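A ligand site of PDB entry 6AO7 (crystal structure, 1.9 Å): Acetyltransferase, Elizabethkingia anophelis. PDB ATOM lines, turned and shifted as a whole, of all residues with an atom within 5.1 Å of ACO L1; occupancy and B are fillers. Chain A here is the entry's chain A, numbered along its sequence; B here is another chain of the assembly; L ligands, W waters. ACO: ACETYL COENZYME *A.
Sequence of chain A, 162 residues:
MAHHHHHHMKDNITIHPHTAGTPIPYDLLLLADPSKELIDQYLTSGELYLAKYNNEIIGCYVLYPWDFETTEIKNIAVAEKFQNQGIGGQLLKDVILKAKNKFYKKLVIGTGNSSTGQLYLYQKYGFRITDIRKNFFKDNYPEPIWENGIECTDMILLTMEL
The backbone NH (N) of Gly 86 lies within hydrogen-bond range of an oxygen (O1A) of ACO L1 (2.8 Å).
The backbone NH (N) of Gly 89 lies within hydrogen-bond range of an oxygen (O2A) of ACO L1 (3.0 Å).
O of ACO L1 lies within hydrogen-bond range of N of Ile 76.
The backbone NH (N) of Gly 88 lies within hydrogen-bond range of an oxygen (O4A) of ACO L1 (2.9 Å).
N of Val 78 lies within hydrogen-bond range of O9P of ACO L1, at 2.8 Å.
O9A of ACO L1 lies within hydrogen-bond range of OH of Tyr 120 (2.6 Å).
The side-chain amide nitrogen (NE2) of Gln 83 sits close to a nitrogen (N8P) of ACO L1, at 3.3 Å.
O5A of ACO L1 lies within hydrogen-bond range of N of Asn 84.
NE2 of Gln 118 is in hydrogen-bond range of O5P of ACO L1 (2.9 Å).
An oxygen (O9A) of ACO L1 is in salt-bridge range of the side-chain amino group of Lys 124.
The backbone carbonyl oxygen (O) of Ile 76 sits at hydrogen-bond distance from a nitrogen (N4P) of ACO L1 (2.8 Å).
The backbone NH of Gln 85 is in hydrogen-bond range of an oxygen (O1A) of ACO L1, 3.3 Å away.
The side-chain amide oxygen (OE1) of Gln 118 lies within hydrogen-bond range of the side-chain hydroxyl (OH) of Tyr 122 (2.7 Å).
The side-chain amide oxygen (OE1) of Gln 118 is in hydrogen-bond range of the side-chain hydroxyl (OG1) of Thr 111 (2.8 Å).
The backbone carbonyl oxygen (O) of Val 78 sits at hydrogen-bond distance from the side-chain amide nitrogen (NE2) of Gln 83, 2.8 Å away.
A sulfur (S1P) of ACO L1 sits close to the backbone carbonyl oxygen (O) of Gly 110, at 3.7 Å.
Merely in contact with ACO L1: Leu 31, Ala 77, Gly 117, Ile 73, Tyr 122, Asn 75, Ala 32, Leu 121, Lys 74, Ile 87, Ile 109 and Thr 111.
Hydrophobic or aromatic side chains within 4 Å of ACO L1: Ala 32, Ile 76, Ala 77, Val 78, Ile 109, Tyr 120 and Leu 121.
Water W6 bridges O4B of ACO L1 and O of Gly 117.
Water W2 bridges O5A of ACO L1 (2.8 Å) and OD1 of Asn 84 (2.9 Å).
Water W7 lies within hydrogen-bond range of a nitrogen (N1A) of ACO L1 (2.8 Å) and a nitrogen (N1A) of ACO L2 (2.8 Å).
Water W4 bridges an oxygen (O2A) of ACO L1 (2.9 Å) and the side-chain amino group (NZ) of Lys 124 (3.2 Å).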
ATOM      1  N   LEU A  31      11.014 -12.206  40.873  1.00  0.00           N
ATOM      2  CA  LEU A  31      11.715 -12.845  39.776  1.00  0.00           C
ATOM      3  C   LEU A  31      12.027 -11.839  38.680  1.00  0.00           C
ATOM      4  O   LEU A  31      13.036 -11.982  37.964  1.00  0.00           O
ATOM      5  CB  LEU A  31      10.890 -13.993  39.185  1.00  0.00           C
ATOM      6  CG  LEU A  31      10.517 -15.166  40.091  1.00  0.00           C
ATOM      7  CD1 LEU A  31       9.585 -16.087  39.320  1.00  0.00           C
ATOM      8  CD2 LEU A  31      11.761 -15.918  40.586  1.00  0.00           C
ATOM      9  N   ALA A  32      11.188 -10.810  38.552  1.00  0.00           N
ATOM     10  CA  ALA A  32      11.308  -9.813  37.496  1.00  0.00           C
ATOM     11  C   ALA A  32      12.006  -8.534  37.953  1.00  0.00           C
ATOM     12  O   ALA A  32      12.545  -7.814  37.111  1.00  0.00           O
ATOM     13  CB  ALA A  32       9.921  -9.467  36.941  1.00  0.00           C
ATOM     14  N   ILE A  73       4.678  -1.659  31.250  1.00  0.00           N
ATOM     15  CA  ILE A  73       4.746  -2.935  31.953  1.00  0.00           C
ATOM     16  C   ILE A  73       5.956  -2.840  32.867  1.00  0.00           C
ATOM     17  O   ILE A  73       7.096  -3.041  32.424  1.00  0.00           O
ATOM     18  CB  ILE A  73       4.870  -4.110  30.985  1.00  0.00           C
ATOM     19  CG1 ILE A  73       3.747  -4.057  29.939  1.00  0.00           C
ATOM     20  CG2 ILE A  73       4.907  -5.448  31.775  1.00  0.00           C
ATOM     21  CD1 ILE A  73       3.889  -5.128  28.865  1.00  0.00           C
ATOM     22  N   LYS A  74       5.727  -2.492  34.145  1.00  0.00           N
ATOM     23  CA  LYS A  74       6.834  -2.382  35.081  1.00  0.00           C
ATOM     24  C   LYS A  74       7.315  -3.738  35.567  1.00  0.00           C
ATOM     25  O   LYS A  74       8.441  -3.843  36.080  1.00  0.00           O
ATOM     26  CB  LYS A  74       6.431  -1.540  36.302  1.00  0.00           C
ATOM     27  CG  LYS A  74       6.664  -0.008  36.184  1.00  0.00           C
ATOM     28  CD  LYS A  74       8.153   0.375  36.250  1.00  0.00           C
ATOM     29  CE  LYS A  74       8.332   1.819  36.731  1.00  0.00           C
ATOM     30  NZ  LYS A  74       9.757   2.274  36.656  1.00  0.00           N
ATOM     31  N   ASN A  75       6.492  -4.774  35.434  1.00  0.00           N
ATOM     32  CA  ASN A  75       6.834  -6.079  35.986  1.00  0.00           C
ATOM     33  C   ASN A  75       6.011  -7.124  35.255  1.00  0.00           C
ATOM     34  O   ASN A  75       4.813  -6.943  35.063  1.00  0.00           O
ATOM     35  CB  ASN A  75       6.552  -6.126  37.501  1.00  0.00           C
ATOM     36  CG  ASN A  75       7.174  -7.341  38.161  1.00  0.00           C
ATOM     37  OD1 ASN A  75       6.807  -8.479  37.858  1.00  0.00           O
ATOM     38  ND2 ASN A  75       8.078  -7.099  39.105  1.00  0.00           N
ATOM     39  N   ILE A  76       6.664  -8.179  34.796  1.00  0.00           N
ATOM     40  CA  ILE A  76       5.950  -9.316  34.229  1.00  0.00           C
ATOM     41  C   ILE A  76       6.740 -10.570  34.575  1.00  0.00           C
ATOM     42  O   ILE A  76       7.963 -10.630  34.367  1.00  0.00           O
ATOM     43  CB  ILE A  76       5.726  -9.195  32.699  1.00  0.00           C
ATOM     44  CG1 ILE A  76       4.882 -10.365  32.187  1.00  0.00           C
ATOM     45  CG2 ILE A  76       7.057  -9.103  31.934  1.00  0.00           C
ATOM     46  CD1 ILE A  76       4.635 -10.322  30.687  1.00  0.00           C
ATOM     47  N   ALA A  77       6.066 -11.563  35.136  1.00  0.00           N
ATOM     48  CA  ALA A  77       6.789 -12.745  35.624  1.00  0.00           C
ATOM     49  C   ALA A  77       5.930 -13.998  35.489  1.00  0.00           C
ATOM     50  O   ALA A  77       4.705 -13.957  35.594  1.00  0.00           O
ATOM     51  CB  ALA A  77       7.219 -12.573  37.082  1.00  0.00           C
ATOM     52  N   VAL A  78       6.616 -15.125  35.272  1.00  0.00           N
ATOM     53  CA  VAL A  78       5.989 -16.438  35.240  1.00  0.00           C
ATOM     54  C   VAL A  78       6.791 -17.340  36.151  1.00  0.00           C
ATOM     55  O   VAL A  78       8.021 -17.346  36.097  1.00  0.00           O
ATOM     56  CB  VAL A  78       5.939 -17.000  33.802  1.00  0.00           C
ATOM     57  CG1 VAL A  78       5.531 -18.455  33.817  1.00  0.00           C
ATOM     58  CG2 VAL A  78       4.994 -16.171  32.952  1.00  0.00           C
ATOM     59  N   PHE A  82       6.919 -23.069  35.364  1.00  0.00           N
ATOM     60  CA  PHE A  82       5.971 -22.946  34.258  1.00  0.00           C
ATOM     61  C   PHE A  82       6.528 -22.112  33.098  1.00  0.00           C
ATOM     62  O   PHE A  82       5.771 -21.799  32.171  1.00  0.00           O
ATOM     63  CB  PHE A  82       4.656 -22.321  34.741  1.00  0.00           C
ATOM     64  CG  PHE A  82       3.878 -23.197  35.659  1.00  0.00           C
ATOM     65  CD1 PHE A  82       2.960 -24.106  35.160  1.00  0.00           C
ATOM     66  CD2 PHE A  82       4.067 -23.122  37.025  1.00  0.00           C
ATOM     67  CE1 PHE A  82       2.236 -24.923  36.014  1.00  0.00           C
ATOM     68  CE2 PHE A  82       3.352 -23.938  37.885  1.00  0.00           C
ATOM     69  CZ  PHE A  82       2.436 -24.835  37.381  1.00  0.00           C
ATOM     70  N   GLN A  83       7.800 -21.741  33.125  1.00  0.00           N
ATOM     71  CA  GLN A  83       8.294 -20.892  32.060  1.00  0.00           C
ATOM     72  C   GLN A  83       8.479 -21.699  30.776  1.00  0.00           C
ATOM     73  O   GLN A  83       8.506 -22.940  30.786  1.00  0.00           O
ATOM     74  CB  GLN A  83       9.607 -20.203  32.476  1.00  0.00           C
ATOM     75  CG  GLN A  83       9.410 -19.019  33.452  1.00  0.00           C
ATOM     76  CD  GLN A  83      10.716 -18.441  33.974  1.00  0.00           C
ATOM     77  OE1 GLN A  83      11.790 -18.715  33.426  1.00  0.00           O
ATOM     78  NE2 GLN A  83      10.626 -17.625  35.015  1.00  0.00           N
ATOM     79  N   ASN A  84       8.591 -20.983  29.653  1.00  0.00           N
ATOM     80  CA  ASN A  84       8.861 -21.579  28.341  1.00  0.00           C
ATOM     81  C   ASN A  84       7.778 -22.578  27.946  1.00  0.00           C
ATOM     82  O   ASN A  84       8.043 -23.587  27.296  1.00  0.00           O
ATOM     83  CB  ASN A  84      10.246 -22.225  28.304  1.00  0.00           C
ATOM     84  CG  ASN A  84      11.336 -21.199  28.386  1.00  0.00           C
ATOM     85  OD1 ASN A  84      11.336 -20.231  27.623  1.00  0.00           O
ATOM     86  ND2 ASN A  84      12.245 -21.361  29.332  1.00  0.00           N
ATOM     87  N   GLN A  85       6.551 -22.282  28.354  1.00  0.00           N
ATOM     88  CA  GLN A  85       5.381 -23.029  27.908  1.00  0.00           C
ATOM     89  C   GLN A  85       4.360 -22.099  27.278  1.00  0.00           C
ATOM     90  O   GLN A  85       3.209 -22.516  27.091  1.00  0.00           O
ATOM     91  CB  GLN A  85       4.747 -23.813  29.061  1.00  0.00           C
ATOM     92  CG  GLN A  85       5.746 -24.392  30.045  1.00  0.00           C
ATOM     93  CD  GLN A  85       5.086 -25.202  31.141  1.00  0.00           C
ATOM     94  OE1 GLN A  85       3.940 -25.635  31.010  1.00  0.00           O
ATOM     95  NE2 GLN A  85       5.808 -25.433  32.233  1.00  0.00           N
ATOM     96  N   GLY A  86       4.735 -20.853  26.960  1.00  0.00           N
ATOM     97  CA  GLY A  86       3.849 -19.906  26.331  1.00  0.00           C
ATOM     98  C   GLY A  86       3.002 -19.056  27.257  1.00  0.00           C
ATOM     99  O   GLY A  86       2.199 -18.251  26.760  1.00  0.00           O
ATOM    100  N   ILE A  87       3.145 -19.180  28.576  1.00  0.00           N
ATOM    101  CA  ILE A  87       2.303 -18.373  29.477  1.00  0.00           C
ATOM    102  C   ILE A  87       2.650 -16.888  29.360  1.00  0.00           C
ATOM    103  O   ILE A  87       1.759 -16.031  29.367  1.00  0.00           O
ATOM    104  CB  ILE A  87       2.427 -18.865  30.926  1.00  0.00           C
ATOM    105  CG1 ILE A  87       1.971 -20.321  31.032  1.00  0.00           C
ATOM    106  CG2 ILE A  87       1.589 -17.979  31.854  1.00  0.00           C
ATOM    107  CD1 ILE A  87       2.192 -20.925  32.394  1.00  0.00           C
ATOM    108  N   GLY A  88       3.937 -16.552  29.256  1.00  0.00           N
ATOM    109  CA  GLY A  88       4.309 -15.155  29.122  1.00  0.00           C
ATOM    110  C   GLY A  88       3.659 -14.482  27.922  1.00  0.00           C
ATOM    111  O   GLY A  88       3.181 -13.352  28.002  1.00  0.00           O
ATOM    112  N   GLY A  89       3.624 -15.186  26.787  1.00  0.00           N
ATOM    113  CA  GLY A  89       2.956 -14.645  25.611  1.00  0.00           C
ATOM    114  C   GLY A  89       1.479 -14.403  25.833  1.00  0.00           C
ATOM    115  O   GLY A  89       0.925 -13.397  25.383  1.00  0.00           O
ATOM    116  N   ILE A 109       7.810  -1.360  27.569  1.00  0.00           N
ATOM    117  CA  ILE A 109       8.448  -2.295  28.493  1.00  0.00           C
ATOM    118  C   ILE A 109       9.959  -2.108  28.406  1.00  0.00           C
ATOM    119  O   ILE A 109      10.511  -1.891  27.328  1.00  0.00           O
ATOM    120  CB  ILE A 109       8.035  -3.750  28.197  1.00  0.00           C
ATOM    121  CG1 ILE A 109       8.495  -4.665  29.327  1.00  0.00           C
ATOM    122  CG2 ILE A 109       8.559  -4.193  26.800  1.00  0.00           C
ATOM    123  CD1 ILE A 109       7.862  -6.060  29.292  1.00  0.00           C
ATOM    124  N   GLY A 110      10.617  -2.169  29.561  1.00  0.00           N
ATOM    125  CA  GLY A 110      12.063  -2.017  29.600  1.00  0.00           C
ATOM    126  C   GLY A 110      12.749  -3.244  30.182  1.00  0.00           C
ATOM    127  O   GLY A 110      12.335  -3.729  31.236  1.00  0.00           O
ATOM    128  N   THR A 111      13.772  -3.764  29.516  1.00  0.00           N
ATOM    129  CA  THR A 111      14.476  -4.920  30.035  1.00  0.00           C
ATOM    130  C   THR A 111      15.983  -4.653  29.971  1.00  0.00           C
ATOM    131  O   THR A 111      16.432  -3.613  29.507  1.00  0.00           O
ATOM    132  CB  THR A 111      14.092  -6.193  29.264  1.00  0.00           C
ATOM    133  OG1 THR A 111      14.579  -7.337  29.979  1.00  0.00           O
ATOM    134  CG2 THR A 111      14.691  -6.161  27.835  1.00  0.00           C
ATOM    135  N   THR A 116      18.817 -10.908  26.181  1.00  0.00           N
ATOM    136  CA  THR A 116      18.631 -11.030  24.748  1.00  0.00           C
ATOM    137  C   THR A 116      17.489 -11.975  24.396  1.00  0.00           C
ATOM    138  O   THR A 116      16.794 -11.750  23.404  1.00  0.00           O
ATOM    139  CB  THR A 116      19.941 -11.456  24.067  1.00  0.00           C
ATOM    140  OG1 THR A 116      20.364 -12.749  24.552  1.00  0.00           O
ATOM    141  CG2 THR A 116      21.027 -10.436  24.348  1.00  0.00           C
ATOM    142  N   GLY A 117      17.257 -13.021  25.198  1.00  0.00           N
ATOM    143  CA  GLY A 117      16.066 -13.831  25.011  1.00  0.00           C
ATOM    144  C   GLY A 117      14.772 -13.042  25.120  1.00  0.00           C
ATOM    145  O   GLY A 117      13.858 -13.216  24.317  1.00  0.00           O
ATOM    146  N   GLN A 118      14.679 -12.172  26.141  1.00  0.00           N
ATOM    147  CA  GLN A 118      13.484 -11.351  26.294  1.00  0.00           C
ATOM    148  C   GLN A 118      13.325 -10.359  25.146  1.00  0.00           C
ATOM    149  O   GLN A 118      12.203 -10.025  24.756  1.00  0.00           O
ATOM    150  CB  GLN A 118      13.530 -10.585  27.616  1.00  0.00           C
ATOM    151  CG  GLN A 118      13.389 -11.441  28.893  1.00  0.00           C
ATOM    152  CD  GLN A 118      13.412 -10.553  30.139  1.00  0.00           C
ATOM    153  OE1 GLN A 118      12.825  -9.482  30.152  1.00  0.00           O
ATOM    154  NE2 GLN A 118      14.141 -10.983  31.172  1.00  0.00           N
ATOM    155  N   TYR A 120      13.882 -10.887  22.115  1.00  0.00           N
ATOM    156  CA  TYR A 120      13.124 -11.629  21.108  1.00  0.00           C
ATOM    157  C   TYR A 120      11.629 -11.634  21.447  1.00  0.00           C
ATOM    158  O   TYR A 120      10.799 -11.261  20.611  1.00  0.00           O
ATOM    159  CB  TYR A 120      13.609 -13.076  20.997  1.00  0.00           C
ATOM    160  CG  TYR A 120      12.562 -13.967  20.355  1.00  0.00           C
ATOM    161  CD1 TYR A 120      12.415 -14.021  18.972  1.00  0.00           C
ATOM    162  CD2 TYR A 120      11.705 -14.731  21.137  1.00  0.00           C
ATOM    163  CE1 TYR A 120      11.435 -14.829  18.389  1.00  0.00           C
ATOM    164  CE2 TYR A 120      10.718 -15.536  20.566  1.00  0.00           C
ATOM    165  CZ  TYR A 120      10.587 -15.566  19.193  1.00  0.00           C
ATOM    166  OH  TYR A 120       9.618 -16.379  18.652  1.00  0.00           O
ATOM    167  N   LEU A 121      11.286 -12.062  22.663  1.00  0.00           N
ATOM    168  CA  LEU A 121       9.883 -12.326  23.000  1.00  0.00           C
ATOM    169  C   LEU A 121       9.028 -11.068  22.842  1.00  0.00           C
ATOM    170  O   LEU A 121       7.932 -11.131  22.264  1.00  0.00           O
ATOM    171  CB  LEU A 121       9.775 -12.876  24.424  1.00  0.00           C
ATOM    172  CG  LEU A 121       8.347 -13.116  24.956  1.00  0.00           C
ATOM    173  CD1 LEU A 121       7.640 -14.174  24.134  1.00  0.00           C
ATOM    174  CD2 LEU A 121       8.392 -13.559  26.422  1.00  0.00           C
ATOM    175  N   TYR A 122       9.492  -9.940  23.368  1.00  0.00           N
ATOM    176  CA  TYR A 122       8.676  -8.732  23.289  1.00  0.00           C
ATOM    177  C   TYR A 122       8.508  -8.287  21.839  1.00  0.00           C
ATOM    178  O   TYR A 122       7.415  -7.865  21.429  1.00  0.00           O
ATOM    179  CB  TYR A 122       9.274  -7.614  24.159  1.00  0.00           C
ATOM    180  CG  TYR A 122       9.504  -8.033  25.618  1.00  0.00           C
ATOM    181  CD1 TYR A 122      10.629  -7.610  26.324  1.00  0.00           C
ATOM    182  CD2 TYR A 122       8.617  -8.858  26.269  1.00  0.00           C
ATOM    183  CE1 TYR A 122      10.873  -8.005  27.625  1.00  0.00           C
ATOM    184  CE2 TYR A 122       8.827  -9.251  27.592  1.00  0.00           C
ATOM    185  CZ  TYR A 122       9.967  -8.808  28.267  1.00  0.00           C
ATOM    186  OH  TYR A 122      10.206  -9.222  29.579  1.00  0.00           O
ATOM    187  N   LYS A 124       8.492 -10.269  19.218  1.00  0.00           N
ATOM    188  CA  LYS A 124       7.529 -11.220  18.657  1.00  0.00           C
ATOM    189  C   LYS A 124       6.091 -10.733  18.848  1.00  0.00           C
ATOM    190  O   LYS A 124       5.235 -10.952  17.983  1.00  0.00           O
ATOM    191  CB  LYS A 124       7.718 -12.598  19.291  1.00  0.00           C
ATOM    192  CG  LYS A 124       6.719 -13.644  18.806  1.00  0.00           C
ATOM    193  CD  LYS A 124       6.659 -14.840  19.765  1.00  0.00           C
ATOM    194  CE  LYS A 124       5.562 -15.822  19.374  1.00  0.00           C
ATOM    195  NZ  LYS A 124       5.555 -17.023  20.255  1.00  0.00           N
ATOM    196  N   THR B 116      19.123 -11.097  17.897  1.00  0.00           N
ATOM    197  CA  THR B 116      19.314 -11.136  19.333  1.00  0.00           C
ATOM    198  C   THR B 116      20.513 -11.990  19.728  1.00  0.00           C
ATOM    199  O   THR B 116      21.191 -11.674  20.708  1.00  0.00           O
ATOM    200  CB  THR B 116      18.031 -11.623  20.039  1.00  0.00           C
ATOM    201  OG1 THR B 116      17.691 -12.949  19.617  1.00  0.00           O
ATOM    202  CG2 THR B 116      16.883 -10.683  19.712  1.00  0.00           C
HETATM  203  N1A ACO L   1      16.788 -16.489  22.678  1.00  0.00           N
HETATM  204  C2A ACO L   1      15.599 -15.910  22.500  1.00  0.00           C
HETATM  205  N3A ACO L   1      14.377 -16.415  22.710  1.00  0.00           N
HETATM  206  C4A ACO L   1      14.452 -17.686  23.123  1.00  0.00           C
HETATM  207  C5A ACO L   1      15.605 -18.434  23.318  1.00  0.00           C
HETATM  208  C6A ACO L   1      16.831 -17.781  23.088  1.00  0.00           C
HETATM  209  N6A ACO L   1      18.026 -18.355  23.234  1.00  0.00           N
HETATM  210  N7A ACO L   1      15.287 -19.732  23.684  1.00  0.00           N
HETATM  211  C8A ACO L   1      13.970 -19.740  23.711  1.00  0.00           C
HETATM  212  N9A ACO L   1      13.402 -18.541  23.378  1.00  0.00           N
HETATM  213  C1B ACO L   1      11.981 -18.219  23.254  1.00  0.00           C
HETATM  214  C2B ACO L   1      11.015 -19.390  23.336  1.00  0.00           C
HETATM  215  O2B ACO L   1      11.003 -20.163  22.143  1.00  0.00           O
HETATM  216  C3B ACO L   1       9.708 -18.617  23.492  1.00  0.00           C
HETATM  217  O3B ACO L   1       9.280 -18.037  22.243  1.00  0.00           O
HETATM  218  P3B ACO L   1       8.259 -18.699  21.192  1.00  0.00           P
HETATM  219  O7A ACO L   1       8.985 -19.925  20.610  1.00  0.00           O
HETATM  220  O8A ACO L   1       6.963 -19.006  21.993  1.00  0.00           O
HETATM  221  O9A ACO L   1       7.981 -17.672  20.135  1.00  0.00           O
HETATM  222  C4B ACO L   1      10.125 -17.379  24.310  1.00  0.00           C
HETATM  223  O4B ACO L   1      11.574 -17.368  24.312  1.00  0.00           O
HETATM  224  C5B ACO L   1       9.559 -17.355  25.714  1.00  0.00           C
HETATM  225  O5B ACO L   1       8.131 -17.457  25.511  1.00  0.00           O
HETATM  226  P1A ACO L   1       7.086 -17.851  26.743  1.00  0.00           P
HETATM  227  O1A ACO L   1       7.049 -19.293  27.082  1.00  0.00           O
HETATM  228  O2A ACO L   1       5.724 -17.332  26.298  1.00  0.00           O
HETATM  229  O3A ACO L   1       7.704 -17.002  27.941  1.00  0.00           O
HETATM  230  P2A ACO L   1       7.614 -17.165  29.531  1.00  0.00           P
HETATM  231  O4A ACO L   1       6.381 -17.950  29.763  1.00  0.00           O
HETATM  232  O5A ACO L   1       8.864 -17.885  30.011  1.00  0.00           O
HETATM  233  O6A ACO L   1       7.607 -15.705  30.148  1.00  0.00           O
HETATM  234  CBP ACO L   1       9.192 -14.193  31.198  1.00  0.00           C
HETATM  235  CCP ACO L   1       8.691 -14.803  29.888  1.00  0.00           C
HETATM  236  CDP ACO L   1       8.047 -13.374  31.813  1.00  0.00           C
HETATM  237  CEP ACO L   1      10.376 -13.266  30.877  1.00  0.00           C
HETATM  238  CAP ACO L   1       9.590 -15.323  32.186  1.00  0.00           C
HETATM  239  OAP ACO L   1      10.564 -16.171  31.596  1.00  0.00           O
HETATM  240  C9P ACO L   1      10.027 -14.858  33.565  1.00  0.00           C
HETATM  241  O9P ACO L   1       9.186 -14.606  34.422  1.00  0.00           O
HETATM  242  N8P ACO L   1      11.323 -14.674  33.754  1.00  0.00           N
HETATM  243  C7P ACO L   1      11.862 -14.135  34.999  1.00  0.00           C
HETATM  244  C6P ACO L   1      11.325 -12.737  35.296  1.00  0.00           C
HETATM  245  C5P ACO L   1      11.668 -11.748  34.205  1.00  0.00           C
HETATM  246  O5P ACO L   1      12.778 -11.743  33.673  1.00  0.00           O
HETATM  247  N4P ACO L   1      10.711 -10.895  33.868  1.00  0.00           N
HETATM  248  C3P ACO L   1      10.883  -9.834  32.878  1.00  0.00           C
HETATM  249  C2P ACO L   1      11.798  -8.736  33.368  1.00  0.00           C
HETATM  250  S1P ACO L   1      11.601  -7.101  32.558  1.00  0.00           S
HETATM  251  C   ACO L   1      10.154  -6.518  33.399  1.00  0.00           C
HETATM  252  O   ACO L   1       9.564  -7.177  34.202  1.00  0.00           O
HETATM  253  CH3 ACO L   1       9.734  -5.145  32.966  1.00  0.00           C
HETATM  254  N1A ACO L   2      21.493 -16.363  21.661  1.00  0.00           N
HETATM  255  C2A ACO L   2      22.644 -15.706  21.808  1.00  0.00           C
HETATM  256  N3A ACO L   2      23.897 -16.146  21.618  1.00  0.00           N
HETATM  257  C4A ACO L   2      23.904 -17.435  21.265  1.00  0.00           C
HETATM  258  C5A ACO L   2      22.798 -18.259  21.112  1.00  0.00           C
HETATM  259  C6A ACO L   2      21.534 -17.677  21.310  1.00  0.00           C
HETATM  260  N6A ACO L   2      20.379 -18.325  21.192  1.00  0.00           N
HETATM  261  N7A ACO L   2      23.202 -19.552  20.801  1.00  0.00           N
HETATM  262  C8A ACO L   2      24.511 -19.482  20.783  1.00  0.00           C
HETATM  263  N9A ACO L   2      25.004 -18.233  21.053  1.00  0.00           N
HETATM  264  C1B ACO L   2      26.402 -17.816  21.159  1.00  0.00           C
HETATM  265  C2B ACO L   2      27.439 -18.919  21.133  1.00  0.00           C
HETATM  266  O2B ACO L   2      27.500 -19.632  22.358  1.00  0.00           O
HETATM  267  C3B ACO L   2      28.696 -18.076  20.937  1.00  0.00           C
HETATM  268  O3B ACO L   2      29.082 -17.412  22.159  1.00  0.00           O
HETATM  269  P3B ACO L   2      30.145 -17.958  23.234  1.00  0.00           P
HETATM  270  O7A ACO L   2      29.490 -19.199  23.867  1.00  0.00           O
HETATM  271  O8A ACO L   2      31.455 -18.220  22.452  1.00  0.00           O
HETATM  272  O9A ACO L   2      30.354 -16.863  24.242  1.00  0.00           O
HETATM  273  C4B ACO L   2      28.202 -16.915  20.063  1.00  0.00           C
HETATM  274  O4B ACO L   2      26.753 -16.997  20.067  1.00  0.00           O
HETATM  275  C5B ACO L   2      28.767 -16.916  18.659  1.00  0.00           C
HETATM  276  O5B ACO L   2      30.199 -16.917  18.864  1.00  0.00           O
HETATM  277  P1A ACO L   2      31.270 -17.306  17.648  1.00  0.00           P
HETATM  278  O1A ACO L   2      31.395 -18.752  17.383  1.00  0.00           O
HETATM  279  O2A ACO L   2      32.583 -16.675  18.067  1.00  0.00           O
HETATM  280  O3A ACO L   2      30.592 -16.553  16.409  1.00  0.00           O
HETATM  281  P2A ACO L   2      30.701 -16.783  14.836  1.00  0.00           P
HETATM  282  O4A ACO L   2      31.982 -17.499  14.639  1.00  0.00           O
HETATM  283  O5A ACO L   2      29.498 -17.600  14.394  1.00  0.00           O
HETATM  284  O6A ACO L   2      30.619 -15.356  14.145  1.00  0.00           O
HETATM  285  CBP ACO L   2      28.941 -13.999  13.032  1.00  0.00           C
HETATM  286  CCP ACO L   2      29.480 -14.516  14.364  1.00  0.00           C
HETATM  287  CDP ACO L   2      30.025 -13.144  12.370  1.00  0.00           C
HETATM  288  CEP ACO L   2      27.699 -13.140  13.314  1.00  0.00           C
HETATM  289  CAP ACO L   2      28.615 -15.201  12.103  1.00  0.00           C
HETATM  290  OAP ACO L   2      27.698 -16.081  12.730  1.00  0.00           O
HETATM  291  C9P ACO L   2      28.154 -14.834  10.701  1.00  0.00           C
HETATM  292  O9P ACO L   2      28.980 -14.575   9.826  1.00  0.00           O
HETATM  293  N8P ACO L   2      26.849 -14.740  10.503  1.00  0.00           N
HETATM  294  C7P ACO L   2      26.279 -14.298   9.236  1.00  0.00           C
HETATM  295  C6P ACO L   2      26.719 -12.881   8.866  1.00  0.00           C
HETATM  296  C5P ACO L   2      26.319 -11.864   9.917  1.00  0.00           C
HETATM  297  O5P ACO L   2      25.213 -11.901  10.445  1.00  0.00           O
HETATM  298  N4P ACO L   2      27.221 -10.940  10.212  1.00  0.00           N
HETATM  299  C3P ACO L   2      26.981  -9.844  11.149  1.00  0.00           C
HETATM  300  C2P ACO L   2      26.000  -8.829  10.606  1.00  0.00           C
HETATM  301  S1P ACO L   2      26.085  -7.150  11.331  1.00  0.00           S
HETATM  302  C   ACO L   2      27.504  -6.520  10.462  1.00  0.00           C
HETATM  303  O   ACO L   2      28.135  -7.177   9.692  1.00  0.00           O
HETATM  304  CH3 ACO L   2      27.834  -5.104  10.834  1.00  0.00           C
HETATM  305  O   HOH W   1      13.791 -15.086  31.746  1.00  0.00           O
HETATM  306  O   HOH W   2      11.345 -17.604  28.837  1.00  0.00           O
HETATM  307  O   HOH W   3      13.359 -16.541  36.500  1.00  0.00           O
HETATM  308  O   HOH W   4       5.267 -17.076  23.489  1.00  0.00           O
HETATM  309  O   HOH W   5       5.346 -20.337  30.054  1.00  0.00           O
HETATM  310  O   HOH W   6      12.525 -15.363  25.255  1.00  0.00           O
HETATM  311  O   HOH W   7      19.094 -14.991  22.138  1.00  0.00           O
